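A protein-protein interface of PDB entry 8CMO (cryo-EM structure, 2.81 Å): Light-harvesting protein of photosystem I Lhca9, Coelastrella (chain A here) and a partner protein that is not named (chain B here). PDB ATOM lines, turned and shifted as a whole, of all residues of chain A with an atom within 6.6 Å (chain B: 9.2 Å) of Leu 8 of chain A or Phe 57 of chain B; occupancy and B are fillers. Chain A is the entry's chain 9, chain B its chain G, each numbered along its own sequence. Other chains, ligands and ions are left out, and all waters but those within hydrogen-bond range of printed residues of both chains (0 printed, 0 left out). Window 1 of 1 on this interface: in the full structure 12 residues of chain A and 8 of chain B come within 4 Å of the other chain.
The backbone carbonyl oxygen (O) of Phe 57 of chain B is in hydrogen-bond range of the side-chain hydroxyl (OG) of Ser 60 of chain B (2.5 Å). The side-chain hydroxyl of Thr 3 of chain A lies within hydrogen-bond range of the backbone carbonyl oxygen of Leu 5 of chain A (2.7 Å). The backbone NH (N) of Trp 4 of chain A is in hydrogen-bond range of the backbone carbonyl oxygen (O) of Phe 22 of chain A (2.9 Å). The backbone carbonyl oxygen (O) of Ser 56 of chain B lies within hydrogen-bond range of the side-chain hydroxyl (OG1) of Thr 59 of chain B, at 2.6 Å. The indole nitrogen (NE1) of Trp 4 of chain A lies within hydrogen-bond range of the backbone carbonyl oxygen (O) of Gly 23 of chain A.
Of chain A, only Trp 4 (3.4 Å), Leu 8 (3.5 Å) and Pro 26 (3.4 Å) come within 4 Å of Phe 57 of chain B. No residue of chain B comes within 4 Å of Gly 23 of chain A. Of the printed residues of chain B, Pro 26 of chain A touches Ala 55 and Phe 57. Of the printed residues of chain B, Asn 7 of chain A touches Ser 60 (2.9 Å). Asp 71 of chain B touches none of the printed residues of chain A. The nearest residue of chain B that does not touch Leu 8 of chain A is Ser 60 of chain B (4.2 Å). The nearest printed residue of chain A that does not touch Thr 59 of chain B is Asn 7 of chain A (5.8 Å).
Printed residues of chain A that touch a printed residue of chain B: Trp 4, Leu 5, Pro 6, Asn 7, Leu 8, Asn 9 and Pro 26. Among the printed residues, no Asp or Glu carboxylate lies within 4 Å of a Lys or Arg side-chain nitrogen of the other chain.
OG1 of Thr 59 of chain B sits at hydrogen-bond distance from ND2 of Asn 9 of chain A (3.5 Å).
Among the printed residues, pairs that only touch across the chains: Asn 7 of chain A with Ser 60 of chain B (2.9 Å), Leu 5 of chain A with Ser 60 of chain B (3.1 Å), Trp 4 of chain A with Phe 57 of chain B (3.4 Å), Pro 26 of chain A with Phe 57 of chain B (3.4 Å), Leu 8 of chain A with Phe 57 of chain B (3.5 Å), Asn 9 of chain A with Ser 56 of chain B (3.6 Å), Leu 5 of chain A with Leu 69 of chain B (3.7 Å), Pro 26 of chain A with Ala 55 of chain B (3.7 Å) and Pro 6 of chain A with Ser 60 of chain B (3.95 Å).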
ATOM      1  N   PRO A   2      17.660 -10.368 -14.244  1.00  0.00           N
ATOM      2  CA  PRO A   2      16.436  -9.556 -14.301  1.00  0.00           C
ATOM      3  C   PRO A   2      16.655  -8.087 -14.700  1.00  0.00           C
ATOM      4  O   PRO A   2      17.603  -7.501 -14.235  1.00  0.00           O
ATOM      5  CB  PRO A   2      15.997  -9.586 -12.837  1.00  0.00           C
ATOM      6  CG  PRO A   2      16.440 -10.932 -12.343  1.00  0.00           C
ATOM      7  CD  PRO A   2      17.788 -11.125 -12.998  1.00  0.00           C
ATOM      8  N   THR A   3      15.764  -7.529 -15.524  1.00  0.00           N
ATOM      9  CA  THR A   3      15.879  -6.100 -15.925  1.00  0.00           C
ATOM     10  C   THR A   3      14.554  -5.378 -15.666  1.00  0.00           C
ATOM     11  O   THR A   3      13.495  -5.972 -15.948  1.00  0.00           O
ATOM     12  CB  THR A   3      16.302  -5.963 -17.393  1.00  0.00           C
ATOM     13  OG1 THR A   3      15.301  -6.585 -18.200  1.00  0.00           O
ATOM     14  CG2 THR A   3      17.652  -6.583 -17.678  1.00  0.00           C
ATOM     15  N   TRP A   4      14.617  -4.143 -15.156  1.00  0.00           N
ATOM     16  CA  TRP A   4      13.386  -3.348 -14.904  1.00  0.00           C
ATOM     17  C   TRP A   4      12.631  -3.171 -16.222  1.00  0.00           C
ATOM     18  O   TRP A   4      11.388  -3.258 -16.210  1.00  0.00           O
ATOM     19  CB  TRP A   4      13.740  -1.996 -14.280  1.00  0.00           C
ATOM     20  CG  TRP A   4      14.436  -1.065 -15.224  1.00  0.00           C
ATOM     21  CD1 TRP A   4      15.780  -0.962 -15.433  1.00  0.00           C
ATOM     22  CD2 TRP A   4      13.821  -0.104 -16.099  1.00  0.00           C
ATOM     23  NE1 TRP A   4      16.044   0.000 -16.370  1.00  0.00           N
ATOM     24  CE2 TRP A   4      14.863   0.542 -16.801  1.00  0.00           C
ATOM     25  CE3 TRP A   4      12.500   0.273 -16.361  1.00  0.00           C
ATOM     26  CZ2 TRP A   4      14.619   1.541 -17.740  1.00  0.00           C
ATOM     27  CZ3 TRP A   4      12.260   1.262 -17.289  1.00  0.00           C
ATOM     28  CH2 TRP A   4      13.307   1.885 -17.968  1.00  0.00           C
ATOM     29  N   LEU A   5      13.364  -2.931 -17.313  1.00  0.00           N
ATOM     30  CA  LEU A   5      12.734  -2.758 -18.645  1.00  0.00           C
ATOM     31  C   LEU A   5      12.804  -4.098 -19.386  1.00  0.00           C
ATOM     32  O   LEU A   5      13.896  -4.693 -19.422  1.00  0.00           O
ATOM     33  CB  LEU A   5      13.491  -1.660 -19.398  1.00  0.00           C
ATOM     34  CG  LEU A   5      12.721  -0.961 -20.517  1.00  0.00           C
ATOM     35  CD1 LEU A   5      12.693  -1.809 -21.778  1.00  0.00           C
ATOM     36  CD2 LEU A   5      11.311  -0.609 -20.070  1.00  0.00           C
ATOM     37  N   PRO A   6      11.695  -4.605 -19.964  1.00  0.00           N
ATOM     38  CA  PRO A   6      11.728  -5.853 -20.728  1.00  0.00           C
ATOM     39  C   PRO A   6      12.716  -5.733 -21.897  1.00  0.00           C
ATOM     40  O   PRO A   6      12.672  -4.735 -22.592  1.00  0.00           O
ATOM     41  CB  PRO A   6      10.290  -6.010 -21.248  1.00  0.00           C
ATOM     42  CG  PRO A   6       9.690  -4.625 -21.134  1.00  0.00           C
ATOM     43  CD  PRO A   6      10.361  -4.007 -19.926  1.00  0.00           C
ATOM     44  N   ASN A   7      13.573  -6.742 -22.081  1.00  0.00           N
ATOM     45  CA  ASN A   7      14.589  -6.703 -23.167  1.00  0.00           C
ATOM     46  C   ASN A   7      15.474  -5.465 -22.984  1.00  0.00           C
ATOM     47  O   ASN A   7      15.659  -4.724 -23.968  1.00  0.00           O
ATOM     48  CB  ASN A   7      13.940  -6.724 -24.554  1.00  0.00           C
ATOM     49  CG  ASN A   7      12.935  -7.843 -24.720  1.00  0.00           C
ATOM     50  OD1 ASN A   7      12.720  -8.633 -23.803  1.00  0.00           O
ATOM     51  ND2 ASN A   7      12.313  -7.919 -25.885  1.00  0.00           N
ATOM     52  N   LEU A   8      15.972  -5.240 -21.764  1.00  0.00           N
ATOM     53  CA  LEU A   8      16.776  -4.021 -21.466  1.00  0.00           C
ATOM     54  C   LEU A   8      18.242  -4.251 -21.844  1.00  0.00           C
ATOM     55  O   LEU A   8      18.610  -5.414 -22.096  1.00  0.00           O
ATOM     56  CB  LEU A   8      16.641  -3.716 -19.970  1.00  0.00           C
ATOM     57  CG  LEU A   8      17.482  -2.555 -19.441  1.00  0.00           C
ATOM     58  CD1 LEU A   8      17.031  -1.238 -20.051  1.00  0.00           C
ATOM     59  CD2 LEU A   8      17.411  -2.491 -17.924  1.00  0.00           C
ATOM     60  N   ASN A   9      19.040  -3.178 -21.878  1.00  0.00           N
ATOM     61  CA  ASN A   9      20.489  -3.295 -22.192  1.00  0.00           C
ATOM     62  C   ASN A   9      21.286  -2.758 -20.999  1.00  0.00           C
ATOM     63  O   ASN A   9      21.753  -1.605 -21.075  1.00  0.00           O
ATOM     64  CB  ASN A   9      20.849  -2.547 -23.476  1.00  0.00           C
ATOM     65  CG  ASN A   9      19.799  -2.682 -24.558  1.00  0.00           C
ATOM     66  OD1 ASN A   9      19.068  -3.669 -24.604  1.00  0.00           O
ATOM     67  ND2 ASN A   9      19.719  -1.696 -25.437  1.00  0.00           N
ATOM     68  N   PRO A  10      21.457  -3.533 -19.904  1.00  0.00           N
ATOM     69  CA  PRO A  10      22.145  -3.045 -18.705  1.00  0.00           C
ATOM     70  C   PRO A  10      23.341  -2.142 -19.035  1.00  0.00           C
ATOM     71  O   PRO A  10      24.255  -2.599 -19.698  1.00  0.00           O
ATOM     72  CB  PRO A  10      22.619  -4.354 -18.059  1.00  0.00           C
ATOM     73  CG  PRO A  10      21.511  -5.331 -18.386  1.00  0.00           C
ATOM     74  CD  PRO A  10      21.012  -4.921 -19.758  1.00  0.00           C
ATOM     75  N   PRO A  11      23.351  -0.870 -18.582  1.00  0.00           N
ATOM     76  CA  PRO A  11      24.476   0.042 -18.823  1.00  0.00           C
ATOM     77  C   PRO A  11      25.785  -0.550 -18.322  1.00  0.00           C
ATOM     78  O   PRO A  11      25.808  -1.352 -17.386  1.00  0.00           O
ATOM     79  CB  PRO A  11      24.084   1.299 -18.039  1.00  0.00           C
ATOM     80  CG  PRO A  11      22.596   1.225 -17.925  1.00  0.00           C
ATOM     81  CD  PRO A  11      22.276  -0.232 -17.806  1.00  0.00           C
ATOM     82  N   PHE A  22      18.943  -4.246 -11.339  1.00  0.00           N
ATOM     83  CA  PHE A  22      17.948  -4.612 -12.373  1.00  0.00           C
ATOM     84  C   PHE A  22      18.232  -3.736 -13.595  1.00  0.00           C
ATOM     85  O   PHE A  22      17.332  -3.541 -14.412  1.00  0.00           O
ATOM     86  CB  PHE A  22      16.535  -4.434 -11.826  1.00  0.00           C
ATOM     87  CG  PHE A  22      16.220  -5.300 -10.637  1.00  0.00           C
ATOM     88  CD1 PHE A  22      16.580  -6.636 -10.621  1.00  0.00           C
ATOM     89  CD2 PHE A  22      15.572  -4.781  -9.532  1.00  0.00           C
ATOM     90  CE1 PHE A  22      16.296  -7.433  -9.525  1.00  0.00           C
ATOM     91  CE2 PHE A  22      15.287  -5.577  -8.434  1.00  0.00           C
ATOM     92  CZ  PHE A  22      15.653  -6.900  -8.435  1.00  0.00           C
ATOM     93  N   GLY A  23      19.450  -3.205 -13.691  1.00  0.00           N
ATOM     94  CA  GLY A  23      19.843  -2.372 -14.837  1.00  0.00           C
ATOM     95  C   GLY A  23      19.092  -1.060 -14.899  1.00  0.00           C
ATOM     96  O   GLY A  23      18.955  -0.545 -16.016  1.00  0.00           O
ATOM     97  N   PHE A  24      18.671  -0.503 -13.756  1.00  0.00           N
ATOM     98  CA  PHE A  24      17.835   0.726 -13.768  1.00  0.00           C
ATOM     99  C   PHE A  24      18.695   1.971 -13.626  1.00  0.00           C
ATOM    100  O   PHE A  24      19.012   2.350 -12.495  1.00  0.00           O
ATOM    101  CB  PHE A  24      16.775   0.705 -12.672  1.00  0.00           C
ATOM    102  CG  PHE A  24      15.791   1.845 -12.677  1.00  0.00           C
ATOM    103  CD1 PHE A  24      14.867   1.979 -13.697  1.00  0.00           C
ATOM    104  CD2 PHE A  24      15.768   2.763 -11.643  1.00  0.00           C
ATOM    105  CE1 PHE A  24      13.949   3.017 -13.691  1.00  0.00           C
ATOM    106  CE2 PHE A  24      14.852   3.802 -11.639  1.00  0.00           C
ATOM    107  CZ  PHE A  24      13.945   3.927 -12.663  1.00  0.00           C
ATOM    108  N   ASP A  25      19.028   2.616 -14.745  1.00  0.00           N
ATOM    109  CA  ASP A  25      19.771   3.904 -14.682  1.00  0.00           C
ATOM    110  C   ASP A  25      19.383   4.723 -15.916  1.00  0.00           C
ATOM    111  O   ASP A  25      20.269   4.996 -16.749  1.00  0.00           O
ATOM    112  CB  ASP A  25      21.280   3.684 -14.542  1.00  0.00           C
ATOM    113  CG  ASP A  25      21.954   4.746 -13.690  1.00  0.00           C
ATOM    114  OD1 ASP A  25      21.266   5.710 -13.304  1.00  0.00           O
ATOM    115  OD2 ASP A  25      23.159   4.596 -13.412  1.00  0.00           O
ATOM    116  N   PRO A  26      18.103   5.135 -16.085  1.00  0.00           N
ATOM    117  CA  PRO A  26      17.685   5.858 -17.288  1.00  0.00           C
ATOM    118  C   PRO A  26      18.598   7.055 -17.579  1.00  0.00           C
ATOM    119  O   PRO A  26      18.682   7.452 -18.727  1.00  0.00           O
ATOM    120  CB  PRO A  26      16.278   6.357 -16.932  1.00  0.00           C
ATOM    121  CG  PRO A  26      15.767   5.330 -15.952  1.00  0.00           C
ATOM    122  CD  PRO A  26      16.988   4.938 -15.148  1.00  0.00           C
ATOM    123  N   LEU A  27      19.247   7.607 -16.549  1.00  0.00           N
ATOM    124  CA  LEU A  27      20.087   8.820 -16.745  1.00  0.00           C
ATOM    125  C   LEU A  27      21.562   8.477 -16.506  1.00  0.00           C
ATOM    126  O   LEU A  27      22.418   9.326 -16.822  1.00  0.00           O
ATOM    127  CB  LEU A  27      19.618   9.914 -15.783  1.00  0.00           C
ATOM    128  CG  LEU A  27      18.167  10.361 -15.947  1.00  0.00           C
ATOM    129  CD1 LEU A  27      17.878  11.574 -15.077  1.00  0.00           C
ATOM    130  CD2 LEU A  27      17.861  10.670 -17.404  1.00  0.00           C
ATOM    131  N   GLN B  53      25.785  11.069 -23.120  1.00  0.00           N
ATOM    132  CA  GLN B  53      25.815   9.890 -24.029  1.00  0.00           C
ATOM    133  C   GLN B  53      24.432   9.230 -24.041  1.00  0.00           C
ATOM    134  O   GLN B  53      23.787   9.208 -22.977  1.00  0.00           O
ATOM    135  CB  GLN B  53      26.903   8.920 -23.570  1.00  0.00           C
ATOM    136  CG  GLN B  53      26.968   7.632 -24.380  1.00  0.00           C
ATOM    137  CD  GLN B  53      27.890   6.628 -23.735  1.00  0.00           C
ATOM    138  OE1 GLN B  53      28.513   6.897 -22.709  1.00  0.00           O
ATOM    139  NE2 GLN B  53      27.978   5.452 -24.332  1.00  0.00           N
ATOM    140  N   GLU B  54      24.009   8.692 -25.190  1.00  0.00           N
ATOM    141  CA  GLU B  54      22.649   8.096 -25.315  1.00  0.00           C
ATOM    142  C   GLU B  54      22.444   6.988 -24.277  1.00  0.00           C
ATOM    143  O   GLU B  54      23.429   6.304 -23.947  1.00  0.00           O
ATOM    144  CB  GLU B  54      22.446   7.550 -26.729  1.00  0.00           C
ATOM    145  CG  GLU B  54      21.944   8.593 -27.710  1.00  0.00           C
ATOM    146  CD  GLU B  54      20.454   8.865 -27.608  1.00  0.00           C
ATOM    147  OE1 GLU B  54      19.731   7.989 -27.094  1.00  0.00           O
ATOM    148  OE2 GLU B  54      20.019   9.953 -28.038  1.00  0.00           O
ATOM    149  N   ALA B  55      21.208   6.819 -23.794  1.00  0.00           N
ATOM    150  CA  ALA B  55      20.891   5.757 -22.806  1.00  0.00           C
ATOM    151  C   ALA B  55      20.809   4.397 -23.513  1.00  0.00           C
ATOM    152  O   ALA B  55      21.580   4.181 -24.465  1.00  0.00           O
ATOM    153  CB  ALA B  55      19.604   6.088 -22.094  1.00  0.00           C
ATOM    154  N   SER B  56      19.906   3.519 -23.060  1.00  0.00           N
ATOM    155  CA  SER B  56      19.757   2.180 -23.692  1.00  0.00           C
ATOM    156  C   SER B  56      18.300   1.709 -23.598  1.00  0.00           C
ATOM    157  O   SER B  56      17.781   1.199 -24.608  1.00  0.00           O
ATOM    158  CB  SER B  56      20.696   1.184 -23.066  1.00  0.00           C
ATOM    159  OG  SER B  56      22.045   1.599 -23.217  1.00  0.00           O
ATOM    160  N   PHE B  57      17.677   1.867 -22.427  1.00  0.00           N
ATOM    161  CA  PHE B  57      16.260   1.459 -22.243  1.00  0.00           C
ATOM    162  C   PHE B  57      15.419   2.020 -23.393  1.00  0.00           C
ATOM    163  O   PHE B  57      14.491   1.330 -23.856  1.00  0.00           O
ATOM    164  CB  PHE B  57      15.734   1.931 -20.885  1.00  0.00           C
ATOM    165  CG  PHE B  57      15.509   3.417 -20.770  1.00  0.00           C
ATOM    166  CD1 PHE B  57      16.568   4.281 -20.549  1.00  0.00           C
ATOM    167  CD2 PHE B  57      14.236   3.952 -20.882  1.00  0.00           C
ATOM    168  CE1 PHE B  57      16.360   5.647 -20.442  1.00  0.00           C
ATOM    169  CE2 PHE B  57      14.029   5.318 -20.775  1.00  0.00           C
ATOM    170  CZ  PHE B  57      15.091   6.163 -20.554  1.00  0.00           C
ATOM    171  N   ILE B  58      15.740   3.238 -23.838  1.00  0.00           N
ATOM    172  CA  ILE B  58      14.977   3.872 -24.954  1.00  0.00           C
ATOM    173  C   ILE B  58      15.130   2.995 -26.201  1.00  0.00           C
ATOM    174  O   ILE B  58      14.149   2.874 -26.951  1.00  0.00           O
ATOM    175  CB  ILE B  58      15.445   5.322 -25.203  1.00  0.00           C
ATOM    176  CG1 ILE B  58      16.717   5.384 -26.053  1.00  0.00           C
ATOM    177  CG2 ILE B  58      15.611   6.068 -23.889  1.00  0.00           C
ATOM    178  CD1 ILE B  58      17.967   4.970 -25.318  1.00  0.00           C
ATOM    179  N   THR B  59      16.305   2.390 -26.393  1.00  0.00           N
ATOM    180  CA  THR B  59      16.563   1.580 -27.615  1.00  0.00           C
ATOM    181  C   THR B  59      16.223   0.109 -27.356  1.00  0.00           C
ATOM    182  O   THR B  59      16.891  -0.759 -27.949  1.00  0.00           O
ATOM    183  CB  THR B  59      18.019   1.722 -28.070  1.00  0.00           C
ATOM    184  OG1 THR B  59      18.855   1.270 -27.004  1.00  0.00           O
ATOM    185  CG2 THR B  59      18.385   3.141 -28.444  1.00  0.00           C
ATOM    186  N   SER B  60      15.204  -0.153 -26.531  1.00  0.00           N
ATOM    187  CA  SER B  60      14.799  -1.550 -26.224  1.00  0.00           C
ATOM    188  C   SER B  60      13.272  -1.684 -26.272  1.00  0.00           C
ATOM    189  O   SER B  60      12.655  -1.754 -25.191  1.00  0.00           O
ATOM    190  CB  SER B  60      15.353  -1.987 -24.894  1.00  0.00           C
ATOM    191  OG  SER B  60      14.912  -1.129 -23.853  1.00  0.00           O
ATOM    192  N   THR B  61      12.694  -1.719 -27.478  1.00  0.00           N
ATOM    193  CA  THR B  61      11.221  -1.882 -27.629  1.00  0.00           C
ATOM    194  C   THR B  61      10.924  -2.904 -28.732  1.00  0.00           C
ATOM    195  O   THR B  61      11.275  -2.628 -29.896  1.00  0.00           O
ATOM    196  CB  THR B  61      10.539  -0.540 -27.921  1.00  0.00           C
ATOM    197  OG1 THR B  61      11.101  -0.003 -29.118  1.00  0.00           O
ATOM    198  CG2 THR B  61      10.694   0.458 -26.794  1.00  0.00           C
ATOM    199  N   ASN B  62      10.297  -4.031 -28.379  1.00  0.00           N
ATOM    200  CA  ASN B  62       9.930  -5.066 -29.384  1.00  0.00           C
ATOM    201  C   ASN B  62       8.873  -4.483 -30.326  1.00  0.00           C
ATOM    202  O   ASN B  62       8.758  -4.977 -31.464  1.00  0.00           O
ATOM    203  CB  ASN B  62       9.440  -6.351 -28.711  1.00  0.00           C
ATOM    204  CG  ASN B  62       9.142  -7.463 -29.693  1.00  0.00           C
ATOM    205  OD1 ASN B  62       8.379  -8.377 -29.387  1.00  0.00           O
ATOM    206  ND2 ASN B  62       9.735  -7.396 -30.873  1.00  0.00           N
ATOM    207  N   PHE B  67       8.675   1.684 -32.114  1.00  0.00           N
ATOM    208  CA  PHE B  67       8.049   2.800 -31.356  1.00  0.00           C
ATOM    209  C   PHE B  67       8.631   2.790 -29.940  1.00  0.00           C
ATOM    210  O   PHE B  67       8.097   2.062 -29.080  1.00  0.00           O
ATOM    211  CB  PHE B  67       6.523   2.679 -31.369  1.00  0.00           C
ATOM    212  CG  PHE B  67       5.785   3.978 -31.177  1.00  0.00           C
ATOM    213  CD1 PHE B  67       5.948   5.024 -32.071  1.00  0.00           C
ATOM    214  CD2 PHE B  67       4.915   4.152 -30.113  1.00  0.00           C
ATOM    215  CE1 PHE B  67       5.267   6.219 -31.900  1.00  0.00           C
ATOM    216  CE2 PHE B  67       4.234   5.348 -29.942  1.00  0.00           C
ATOM    217  CZ  PHE B  67       4.411   6.378 -30.836  1.00  0.00           C
ATOM    218  N   THR B  68       9.687   3.574 -29.708  1.00  0.00           N
ATOM    219  CA  THR B  68      10.382   3.560 -28.391  1.00  0.00           C
ATOM    220  C   THR B  68       9.516   4.217 -27.311  1.00  0.00           C
ATOM    221  O   THR B  68       8.561   4.931 -27.674  1.00  0.00           O
ATOM    222  CB  THR B  68      11.745   4.250 -28.497  1.00  0.00           C
ATOM    223  OG1 THR B  68      11.511   5.613 -28.849  1.00  0.00           O
ATOM    224  CG2 THR B  68      12.648   3.607 -29.526  1.00  0.00           C
ATOM    225  N   LEU B  69       9.853   3.990 -26.038  1.00  0.00           N
ATOM    226  CA  LEU B  69       9.085   4.587 -24.914  1.00  0.00           C
ATOM    227  C   LEU B  69       9.077   6.110 -25.076  1.00  0.00           C
ATOM    228  O   LEU B  69       8.024   6.724 -24.826  1.00  0.00           O
ATOM    229  CB  LEU B  69       9.739   4.196 -23.585  1.00  0.00           C
ATOM    230  CG  LEU B  69      10.060   2.714 -23.405  1.00  0.00           C
ATOM    231  CD1 LEU B  69      11.444   2.392 -23.945  1.00  0.00           C
ATOM    232  CD2 LEU B  69       9.968   2.320 -21.938  1.00  0.00           C
ATOM    233  N   ILE B  70      10.213   6.687 -25.474  1.00  0.00           N
ATOM    234  CA  ILE B  70      10.303   8.167 -25.653  1.00  0.00           C
ATOM    235  C   ILE B  70       9.286   8.587 -26.719  1.00  0.00           C
ATOM    236  O   ILE B  70       8.635   9.629 -26.525  1.00  0.00           O
ATOM    237  CB  ILE B  70      11.741   8.601 -26.001  1.00  0.00           C
ATOM    238  CG1 ILE B  70      12.189   8.080 -27.369  1.00  0.00           C
ATOM    239  CG2 ILE B  70      12.706   8.190 -24.901  1.00  0.00           C
ATOM    240  CD1 ILE B  70      13.639   8.360 -27.687  1.00  0.00           C
ATOM    241  N   ASP B  71       9.143   7.795 -27.787  1.00  0.00           N
ATOM    242  CA  ASP B  71       8.153   8.104 -28.854  1.00  0.00           C
ATOM    243  C   ASP B  71       6.738   8.025 -28.271  1.00  0.00           C
ATOM    244  O   ASP B  71       5.925   8.919 -28.578  1.00  0.00           O
ATOM    245  CB  ASP B  71       8.315   7.177 -30.060  1.00  0.00           C
ATOM    246  CG  ASP B  71       9.546   7.491 -30.893  1.00  0.00           C
ATOM    247  OD1 ASP B  71      10.636   7.612 -30.303  1.00  0.00           O
ATOM    248  OD2 ASP B  71       9.397   7.629 -32.122  1.00  0.00           O
ATOM    249  N   MET B  73       5.902   8.466 -25.173  1.00  0.00           N
ATOM    250  CA  MET B  73       5.763   9.614 -24.237  1.00  0.00           C
ATOM    251  C   MET B  73       5.844  10.924 -25.026  1.00  0.00           C
ATOM    252  O   MET B  73       5.579  11.982 -24.431  1.00  0.00           O
ATOM    253  CB  MET B  73       6.872   9.592 -23.182  1.00  0.00           C
ATOM    254  CG  MET B  73       6.816   8.380 -22.274  1.00  0.00           C
ATOM    255  SD  MET B  73       8.181   8.346 -21.087  1.00  0.00           S
ATOM    256  CE  MET B  73       9.577   8.182 -22.198  1.00  0.00           C
